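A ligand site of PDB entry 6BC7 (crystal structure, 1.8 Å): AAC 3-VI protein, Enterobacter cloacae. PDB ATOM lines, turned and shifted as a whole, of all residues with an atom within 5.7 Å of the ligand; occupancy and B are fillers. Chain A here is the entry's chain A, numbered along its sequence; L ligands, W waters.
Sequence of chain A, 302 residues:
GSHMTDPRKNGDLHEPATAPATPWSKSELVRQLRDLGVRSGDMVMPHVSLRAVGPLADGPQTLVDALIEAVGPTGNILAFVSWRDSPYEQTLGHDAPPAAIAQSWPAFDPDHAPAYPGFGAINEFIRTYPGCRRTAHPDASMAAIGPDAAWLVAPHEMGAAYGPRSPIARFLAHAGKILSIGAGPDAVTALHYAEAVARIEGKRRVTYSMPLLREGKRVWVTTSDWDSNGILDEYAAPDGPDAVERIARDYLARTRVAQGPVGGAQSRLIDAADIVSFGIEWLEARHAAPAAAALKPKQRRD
Residues that only touch the ligand: Phe 80 (3.99 Å), Ser 82 (3.2 Å), Trp 83 (3.9 Å), Tyr 88 (3.3 Å), Tyr 116 (3.2 Å), Phe 119 (3.6 Å) and Asp 242 (3.3 Å).
Hydrophobic or aromatic side chains within 4 Å of the ligand: Phe 80, Tyr 88, Tyr 116, Phe 119, Tyr 162 and His 192.
Along chain A the residues within 4 Å of the ligand span positions 80 to 242.
The nearest printed residue that does not touch the ligand is Ser 86 (4.02 Å).
The side-chain hydroxyl (OG) of Ser 228 lies within hydrogen-bond range of a nitrogen (N1) of the ligand (2.8 Å).
A nitrogen (N4) of the ligand lies within salt-bridge range of the side-chain carboxylate of Asp 139.
A ring nitrogen (NE2) of His 192 sits at hydrogen-bond distance from a nitrogen (N3) of the ligand (2.7 Å).
An oxygen (O5) of the ligand lies within hydrogen-bond range of the side-chain amide oxygen (OD1) of Asn 229 (2.7 Å).
OH of Tyr 162 sits at hydrogen-bond distance from N1 of the ligand (2.8 Å).
N2 of the ligand lies within salt-bridge range of OD2 of Asp 186 (2.7 Å).
Water W2 bridges a nitrogen (N5) of the ligand (2.6 Å) and the backbone carbonyl oxygen of Asn 229 (2.9 Å).
Water W6 bridges a nitrogen (N4) of the ligand and the backbone carbonyl oxygen of Ser 86.
Water W1 lies within hydrogen-bond range of the side-chain carboxylate of Asp 242 (2.6 Å), the backbone carbonyl oxygen of Asp 186 (2.8 Å) and a nitrogen (N3) of the ligand (2.9 Å).
The backbone NH of Val 244 lies close to the side-chain carboxylate of Asp 242 (3.5 Å).
The side-chain hydroxyl of Ser 86 is in hydrogen-bond range of the side-chain carboxylate of Asp 139 (2.6 Å).
The backbone carbonyl oxygen of Asp 139 is in hydrogen-bond range of the side-chain hydroxyl of Ser 82.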
ATOM      1  N   PHE A  80     -28.251 -18.192  28.497  1.00  0.00           N
ATOM      2  CA  PHE A  80     -26.935 -18.644  28.064  1.00  0.00           C
ATOM      3  C   PHE A  80     -26.278 -19.353  29.245  1.00  0.00           C
ATOM      4  O   PHE A  80     -25.897 -18.697  30.228  1.00  0.00           O
ATOM      5  CB  PHE A  80     -26.122 -17.452  27.566  1.00  0.00           C
ATOM      6  CG  PHE A  80     -24.654 -17.753  27.415  1.00  0.00           C
ATOM      7  CD1 PHE A  80     -23.695 -16.957  28.051  1.00  0.00           C
ATOM      8  CD2 PHE A  80     -24.247 -18.836  26.636  1.00  0.00           C
ATOM      9  CE1 PHE A  80     -22.320 -17.253  27.905  1.00  0.00           C
ATOM     10  CE2 PHE A  80     -22.888 -19.141  26.506  1.00  0.00           C
ATOM     11  CZ  PHE A  80     -21.932 -18.335  27.132  1.00  0.00           C
ATOM     12  N   SER A  82     -23.970 -22.371  28.837  1.00  0.00           N
ATOM     13  CA  SER A  82     -22.645 -22.938  28.500  1.00  0.00           C
ATOM     14  C   SER A  82     -22.497 -24.295  29.203  1.00  0.00           C
ATOM     15  O   SER A  82     -23.484 -25.006  29.413  1.00  0.00           O
ATOM     16  CB  SER A  82     -21.552 -21.925  28.858  1.00  0.00           C
ATOM     17  OG  SER A  82     -20.273 -22.387  28.405  1.00  0.00           O
ATOM     18  N   TRP A  83     -21.271 -24.629  29.611  1.00  0.00           N
ATOM     19  CA  TRP A  83     -20.979 -25.941  30.187  1.00  0.00           C
ATOM     20  C   TRP A  83     -19.812 -25.795  31.160  1.00  0.00           C
ATOM     21  O   TRP A  83     -18.776 -25.237  30.787  1.00  0.00           O
ATOM     22  CB  TRP A  83     -20.620 -26.923  29.063  1.00  0.00           C
ATOM     23  CG  TRP A  83     -20.237 -28.299  29.491  1.00  0.00           C
ATOM     24  CD1 TRP A  83     -20.520 -28.932  30.675  1.00  0.00           C
ATOM     25  CD2 TRP A  83     -19.512 -29.237  28.698  1.00  0.00           C
ATOM     26  NE1 TRP A  83     -20.005 -30.221  30.666  1.00  0.00           N
ATOM     27  CE2 TRP A  83     -19.378 -30.419  29.458  1.00  0.00           C
ATOM     28  CE3 TRP A  83     -18.972 -29.195  27.420  1.00  0.00           C
ATOM     29  CZ2 TRP A  83     -18.718 -31.556  28.964  1.00  0.00           C
ATOM     30  CZ3 TRP A  83     -18.305 -30.301  26.943  1.00  0.00           C
ATOM     31  CH2 TRP A  83     -18.189 -31.461  27.707  1.00  0.00           C
ATOM     32  N   SER A  86     -16.540 -27.298  29.602  1.00  0.00           N
ATOM     33  CA  SER A  86     -16.236 -27.102  28.185  1.00  0.00           C
ATOM     34  C   SER A  86     -14.722 -27.128  27.986  1.00  0.00           C
ATOM     35  O   SER A  86     -14.001 -26.406  28.683  1.00  0.00           O
ATOM     36  CB  SER A  86     -16.807 -25.771  27.687  1.00  0.00           C
ATOM     37  OG  SER A  86     -16.257 -25.428  26.411  1.00  0.00           O
ATOM     38  N   TYR A  88     -12.669 -25.582  26.256  1.00  0.00           N
ATOM     39  CA  TYR A  88     -12.359 -24.439  25.383  1.00  0.00           C
ATOM     40  C   TYR A  88     -10.874 -24.109  25.404  1.00  0.00           C
ATOM     41  O   TYR A  88     -10.188 -24.197  24.382  1.00  0.00           O
ATOM     42  CB  TYR A  88     -13.196 -23.227  25.819  1.00  0.00           C
ATOM     43  CG  TYR A  88     -13.097 -21.983  24.949  1.00  0.00           C
ATOM     44  CD1 TYR A  88     -13.953 -21.820  23.861  1.00  0.00           C
ATOM     45  CD2 TYR A  88     -12.183 -20.967  25.222  1.00  0.00           C
ATOM     46  CE1 TYR A  88     -13.890 -20.680  23.069  1.00  0.00           C
ATOM     47  CE2 TYR A  88     -12.112 -19.827  24.427  1.00  0.00           C
ATOM     48  CZ  TYR A  88     -12.985 -19.692  23.356  1.00  0.00           C
ATOM     49  OH  TYR A  88     -12.932 -18.574  22.536  1.00  0.00           O
ATOM     50  N   GLU A  89     -10.355 -23.698  26.568  1.00  0.00           N
ATOM     51  CA  GLU A  89      -8.937 -23.371  26.650  1.00  0.00           C
ATOM     52  C   GLU A  89      -8.067 -24.570  26.287  1.00  0.00           C
ATOM     53  O   GLU A  89      -6.980 -24.419  25.711  1.00  0.00           O
ATOM     54  CB  GLU A  89      -8.567 -22.879  28.040  1.00  0.00           C
ATOM     55  CG  GLU A  89      -9.067 -21.491  28.341  1.00  0.00           C
ATOM     56  CD  GLU A  89      -8.485 -20.425  27.415  1.00  0.00           C
ATOM     57  OE1 GLU A  89      -9.206 -19.435  27.133  1.00  0.00           O
ATOM     58  OE2 GLU A  89      -7.314 -20.569  26.987  1.00  0.00           O
ATOM     59  N   TYR A 116     -22.079 -23.598  33.211  1.00  0.00           N
ATOM     60  CA  TYR A 116     -20.860 -22.919  33.613  1.00  0.00           C
ATOM     61  C   TYR A 116     -21.161 -21.949  34.763  1.00  0.00           C
ATOM     62  O   TYR A 116     -21.943 -21.020  34.573  1.00  0.00           O
ATOM     63  CB  TYR A 116     -20.257 -22.152  32.425  1.00  0.00           C
ATOM     64  CG  TYR A 116     -18.896 -21.586  32.730  1.00  0.00           C
ATOM     65  CD1 TYR A 116     -17.776 -22.421  32.767  1.00  0.00           C
ATOM     66  CD2 TYR A 116     -18.717 -20.235  32.976  1.00  0.00           C
ATOM     67  CE1 TYR A 116     -16.506 -21.922  33.059  1.00  0.00           C
ATOM     68  CE2 TYR A 116     -17.429 -19.718  33.251  1.00  0.00           C
ATOM     69  CZ  TYR A 116     -16.348 -20.570  33.300  1.00  0.00           C
ATOM     70  OH  TYR A 116     -15.092 -20.081  33.586  1.00  0.00           O
ATOM     71  N   PHE A 119     -21.340 -17.798  34.585  1.00  0.00           N
ATOM     72  CA  PHE A 119     -22.368 -17.030  33.891  1.00  0.00           C
ATOM     73  C   PHE A 119     -23.659 -16.956  34.689  1.00  0.00           C
ATOM     74  O   PHE A 119     -24.691 -16.550  34.139  1.00  0.00           O
ATOM     75  CB  PHE A 119     -22.650 -17.626  32.502  1.00  0.00           C
ATOM     76  CG  PHE A 119     -21.433 -17.711  31.631  1.00  0.00           C
ATOM     77  CD1 PHE A 119     -20.484 -16.692  31.655  1.00  0.00           C
ATOM     78  CD2 PHE A 119     -21.229 -18.807  30.796  1.00  0.00           C
ATOM     79  CE1 PHE A 119     -19.355 -16.757  30.870  1.00  0.00           C
ATOM     80  CE2 PHE A 119     -20.087 -18.874  29.987  1.00  0.00           C
ATOM     81  CZ  PHE A 119     -19.146 -17.864  30.024  1.00  0.00           C
ATOM     82  N   ASP A 139     -20.018 -25.291  24.129  1.00  0.00           N
ATOM     83  CA  ASP A 139     -19.467 -24.085  24.734  1.00  0.00           C
ATOM     84  C   ASP A 139     -20.456 -22.920  24.790  1.00  0.00           C
ATOM     85  O   ASP A 139     -20.419 -22.119  25.738  1.00  0.00           O
ATOM     86  CB  ASP A 139     -18.213 -23.652  23.983  1.00  0.00           C
ATOM     87  CG  ASP A 139     -17.430 -22.628  24.751  1.00  0.00           C
ATOM     88  OD1 ASP A 139     -16.935 -22.985  25.825  1.00  0.00           O
ATOM     89  OD2 ASP A 139     -17.364 -21.456  24.299  1.00  0.00           O
ATOM     90  N   ALA A 140     -21.321 -22.801  23.790  1.00  0.00           N
ATOM     91  CA  ALA A 140     -22.304 -21.726  23.703  1.00  0.00           C
ATOM     92  C   ALA A 140     -23.689 -22.170  24.179  1.00  0.00           C
ATOM     93  O   ALA A 140     -24.683 -21.466  23.915  1.00  0.00           O
ATOM     94  CB  ALA A 140     -22.372 -21.202  22.260  1.00  0.00           C
ATOM     95  N   TYR A 162     -23.111 -17.619  18.429  1.00  0.00           N
ATOM     96  CA  TYR A 162     -23.967 -16.498  18.824  1.00  0.00           C
ATOM     97  C   TYR A 162     -24.477 -15.665  17.657  1.00  0.00           C
ATOM     98  O   TYR A 162     -25.187 -14.692  17.903  1.00  0.00           O
ATOM     99  CB  TYR A 162     -23.236 -15.549  19.797  1.00  0.00           C
ATOM    100  CG  TYR A 162     -22.572 -16.291  20.936  1.00  0.00           C
ATOM    101  CD1 TYR A 162     -21.180 -16.499  20.938  1.00  0.00           C
ATOM    102  CD2 TYR A 162     -23.328 -16.799  21.998  1.00  0.00           C
ATOM    103  CE1 TYR A 162     -20.569 -17.216  21.956  1.00  0.00           C
ATOM    104  CE2 TYR A 162     -22.712 -17.545  23.037  1.00  0.00           C
ATOM    105  CZ  TYR A 162     -21.341 -17.734  23.001  1.00  0.00           C
ATOM    106  OH  TYR A 162     -20.728 -18.453  23.987  1.00  0.00           O
ATOM    107  N   ASP A 186     -21.328  -5.946  31.034  1.00  0.00           N
ATOM    108  CA  ASP A 186     -20.604  -6.954  30.255  1.00  0.00           C
ATOM    109  C   ASP A 186     -21.438  -8.203  30.023  1.00  0.00           C
ATOM    110  O   ASP A 186     -21.138  -8.987  29.124  1.00  0.00           O
ATOM    111  CB  ASP A 186     -19.325  -7.342  30.974  1.00  0.00           C
ATOM    112  CG  ASP A 186     -19.615  -8.026  32.297  1.00  0.00           C
ATOM    113  OD1 ASP A 186     -20.102  -7.351  33.223  1.00  0.00           O
ATOM    114  OD2 ASP A 186     -19.387  -9.254  32.398  1.00  0.00           O
ATOM    115  N   ALA A 187     -22.464  -8.412  30.833  1.00  0.00           N
ATOM    116  CA  ALA A 187     -23.257  -9.643  30.745  1.00  0.00           C
ATOM    117  C   ALA A 187     -24.464  -9.400  29.868  1.00  0.00           C
ATOM    118  O   ALA A 187     -25.608  -9.314  30.333  1.00  0.00           O
ATOM    119  CB  ALA A 187     -23.678 -10.096  32.135  1.00  0.00           C
ATOM    120  N   THR A 189     -25.108 -11.245  26.552  1.00  0.00           N
ATOM    121  CA  THR A 189     -24.594 -12.206  25.570  1.00  0.00           C
ATOM    122  C   THR A 189     -25.121 -11.928  24.176  1.00  0.00           C
ATOM    123  O   THR A 189     -24.436 -12.194  23.194  1.00  0.00           O
ATOM    124  CB  THR A 189     -24.978 -13.623  26.021  1.00  0.00           C
ATOM    125  OG1 THR A 189     -24.644 -13.772  27.400  1.00  0.00           O
ATOM    126  CG2 THR A 189     -24.221 -14.676  25.183  1.00  0.00           C
ATOM    127  N   HIS A 192     -23.095 -10.452  21.323  1.00  0.00           N
ATOM    128  CA  HIS A 192     -22.191 -11.214  20.460  1.00  0.00           C
ATOM    129  C   HIS A 192     -22.792 -11.444  19.071  1.00  0.00           C
ATOM    130  O   HIS A 192     -22.045 -11.711  18.123  1.00  0.00           O
ATOM    131  CB  HIS A 192     -21.805 -12.577  21.085  1.00  0.00           C
ATOM    132  CG  HIS A 192     -21.042 -12.472  22.373  1.00  0.00           C
ATOM    133  ND1 HIS A 192     -19.871 -11.749  22.483  1.00  0.00           N
ATOM    134  CD2 HIS A 192     -21.312 -12.962  23.608  1.00  0.00           C
ATOM    135  CE1 HIS A 192     -19.459 -11.789  23.742  1.00  0.00           C
ATOM    136  NE2 HIS A 192     -20.303 -12.537  24.435  1.00  0.00           N
ATOM    137  N   SER A 228     -15.518 -14.736  21.120  1.00  0.00           N
ATOM    138  CA  SER A 228     -16.510 -14.179  22.018  1.00  0.00           C
ATOM    139  C   SER A 228     -15.881 -13.519  23.253  1.00  0.00           C
ATOM    140  O   SER A 228     -16.592 -13.104  24.183  1.00  0.00           O
ATOM    141  CB  SER A 228     -17.518 -15.268  22.430  1.00  0.00           C
ATOM    142  OG  SER A 228     -16.896 -16.281  23.221  1.00  0.00           O
ATOM    143  N   ASN A 229     -14.543 -13.401  23.285  1.00  0.00           N
ATOM    144  CA  ASN A 229     -13.863 -12.607  24.301  1.00  0.00           C
ATOM    145  C   ASN A 229     -13.289 -11.316  23.741  1.00  0.00           C
ATOM    146  O   ASN A 229     -12.224 -10.870  24.167  1.00  0.00           O
ATOM    147  CB  ASN A 229     -12.776 -13.431  24.961  1.00  0.00           C
ATOM    148  CG  ASN A 229     -13.360 -14.465  25.906  1.00  0.00           C
ATOM    149  OD1 ASN A 229     -14.093 -14.099  26.844  1.00  0.00           O
ATOM    150  ND2 ASN A 229     -13.097 -15.740  25.625  1.00  0.00           N
ATOM    151  N   GLY A 230     -13.961 -10.725  22.757  1.00  0.00           N
ATOM    152  CA  GLY A 230     -13.530  -9.468  22.177  1.00  0.00           C
ATOM    153  C   GLY A 230     -13.417  -9.570  20.673  1.00  0.00           C
ATOM    154  O   GLY A 230     -12.533 -10.267  20.166  1.00  0.00           O
ATOM    155  N   GLY A 240      -9.245  -5.114  30.475  1.00  0.00           N
ATOM    156  CA  GLY A 240     -10.051  -3.989  30.043  1.00  0.00           C
ATOM    157  C   GLY A 240     -11.429  -4.441  29.613  1.00  0.00           C
ATOM    158  O   GLY A 240     -11.697  -5.632  29.457  1.00  0.00           O
ATOM    159  N   ASP A 242     -14.624  -5.315  27.325  1.00  0.00           N
ATOM    160  CA  ASP A 242     -14.785  -5.903  25.996  1.00  0.00           C
ATOM    161  C   ASP A 242     -15.799  -5.083  25.191  1.00  0.00           C
ATOM    162  O   ASP A 242     -16.278  -4.047  25.649  1.00  0.00           O
ATOM    163  CB  ASP A 242     -15.153  -7.393  26.112  1.00  0.00           C
ATOM    164  CG  ASP A 242     -16.511  -7.638  26.748  1.00  0.00           C
ATOM    165  OD1 ASP A 242     -16.896  -8.827  26.843  1.00  0.00           O
ATOM    166  OD2 ASP A 242     -17.159  -6.666  27.174  1.00  0.00           O
ATOM    167  N   VAL A 244     -18.797  -5.894  24.186  1.00  0.00           N
ATOM    168  CA  VAL A 244     -20.127  -6.002  24.776  1.00  0.00           C
ATOM    169  C   VAL A 244     -20.319  -4.942  25.849  1.00  0.00           C
ATOM    170  O   VAL A 244     -21.304  -4.183  25.830  1.00  0.00           O
ATOM    171  CB  VAL A 244     -20.372  -7.409  25.353  1.00  0.00           C
ATOM    172  CG1 VAL A 244     -21.674  -7.456  26.140  1.00  0.00           C
ATOM    173  CG2 VAL A 244     -20.366  -8.472  24.249  1.00  0.00           C
HETATM  174  C1  LIG L   1     -17.106 -12.709  29.990  1.00  0.00           C
HETATM  175  C2  LIG L   1     -18.502 -16.397  26.470  1.00  0.00           C
HETATM  176  C3  LIG L   1     -15.653 -18.176  26.699  1.00  0.00           C
HETATM  177  C4  LIG L   1     -17.610 -12.028  31.003  1.00  0.00           C
HETATM  178  C5  LIG L   1     -19.152 -15.005  26.085  1.00  0.00           C
HETATM  179  C6  LIG L   1     -15.989 -19.679  26.786  1.00  0.00           C
HETATM  180  C7  LIG L   1     -16.460 -11.055  31.722  1.00  0.00           C
HETATM  181  C8  LIG L   1     -19.254 -14.067  27.357  1.00  0.00           C
HETATM  182  C9  LIG L   1     -15.932 -20.152  28.219  1.00  0.00           C
HETATM  183  C10 LIG L   1     -15.624 -10.397  30.870  1.00  0.00           C
HETATM  184  C11 LIG L   1     -17.859 -13.950  28.038  1.00  0.00           C
HETATM  185  C12 LIG L   1     -14.626 -19.803  28.862  1.00  0.00           C
HETATM  186  C13 LIG L   1     -15.533 -10.839  29.368  1.00  0.00           C
HETATM  187  C14 LIG L   1     -17.086 -15.323  28.190  1.00  0.00           C
HETATM  188  C15 LIG L   1     -14.292 -18.295  28.692  1.00  0.00           C
HETATM  189  C16 LIG L   1     -14.400 -10.330  28.460  1.00  0.00           C
HETATM  190  C17 LIG L   1     -17.112 -16.232  26.973  1.00  0.00           C
HETATM  191  C18 LIG L   1     -14.583 -20.139  30.396  1.00  0.00           C
HETATM  192  C19 LIG L   1     -17.157 -22.049  29.160  1.00  0.00           C
HETATM  193  N1  LIG L   1     -18.513 -17.323  25.312  1.00  0.00           N
HETATM  194  N2  LIG L   1     -18.794 -11.145  30.577  1.00  0.00           N
HETATM  195  N3  LIG L   1     -19.722 -12.737  27.079  1.00  0.00           N
HETATM  196  N4  LIG L   1     -16.109 -21.672  28.168  1.00  0.00           N
HETATM  197  N5  LIG L   1     -13.593 -11.516  28.093  1.00  0.00           N
HETATM  198  O1  LIG L   1     -18.176 -13.472  29.321  1.00  0.00           O
HETATM  199  O2  LIG L   1     -17.297 -19.880  26.251  1.00  0.00           O
HETATM  200  O3  LIG L   1     -13.594 -20.576  28.234  1.00  0.00           O
HETATM  201  O4  LIG L   1     -16.399 -11.811  28.881  1.00  0.00           O
HETATM  202  O5  LIG L   1     -15.764 -15.136  28.670  1.00  0.00           O
HETATM  203  O6  LIG L   1     -14.297 -17.946  27.251  1.00  0.00           O
HETATM  204  O7  LIG L   1     -16.594 -17.540  27.464  1.00  0.00           O
HETATM  205  O   HOH W   1     -18.922 -10.041  27.811  1.00  0.00           O
HETATM  206  O   HOH W   2     -11.658 -10.311  26.913  1.00  0.00           O
HETATM  207  O   HOH W   3     -11.343 -20.291  29.851  1.00  0.00           O
HETATM  208  O   HOH W   4     -13.628  -7.387  30.039  1.00  0.00           O
HETATM  209  O   HOH W   5     -15.113 -15.826  31.236  1.00  0.00           O
HETATM  210  O   HOH W   6     -14.417 -23.449  29.433  1.00  0.00           O
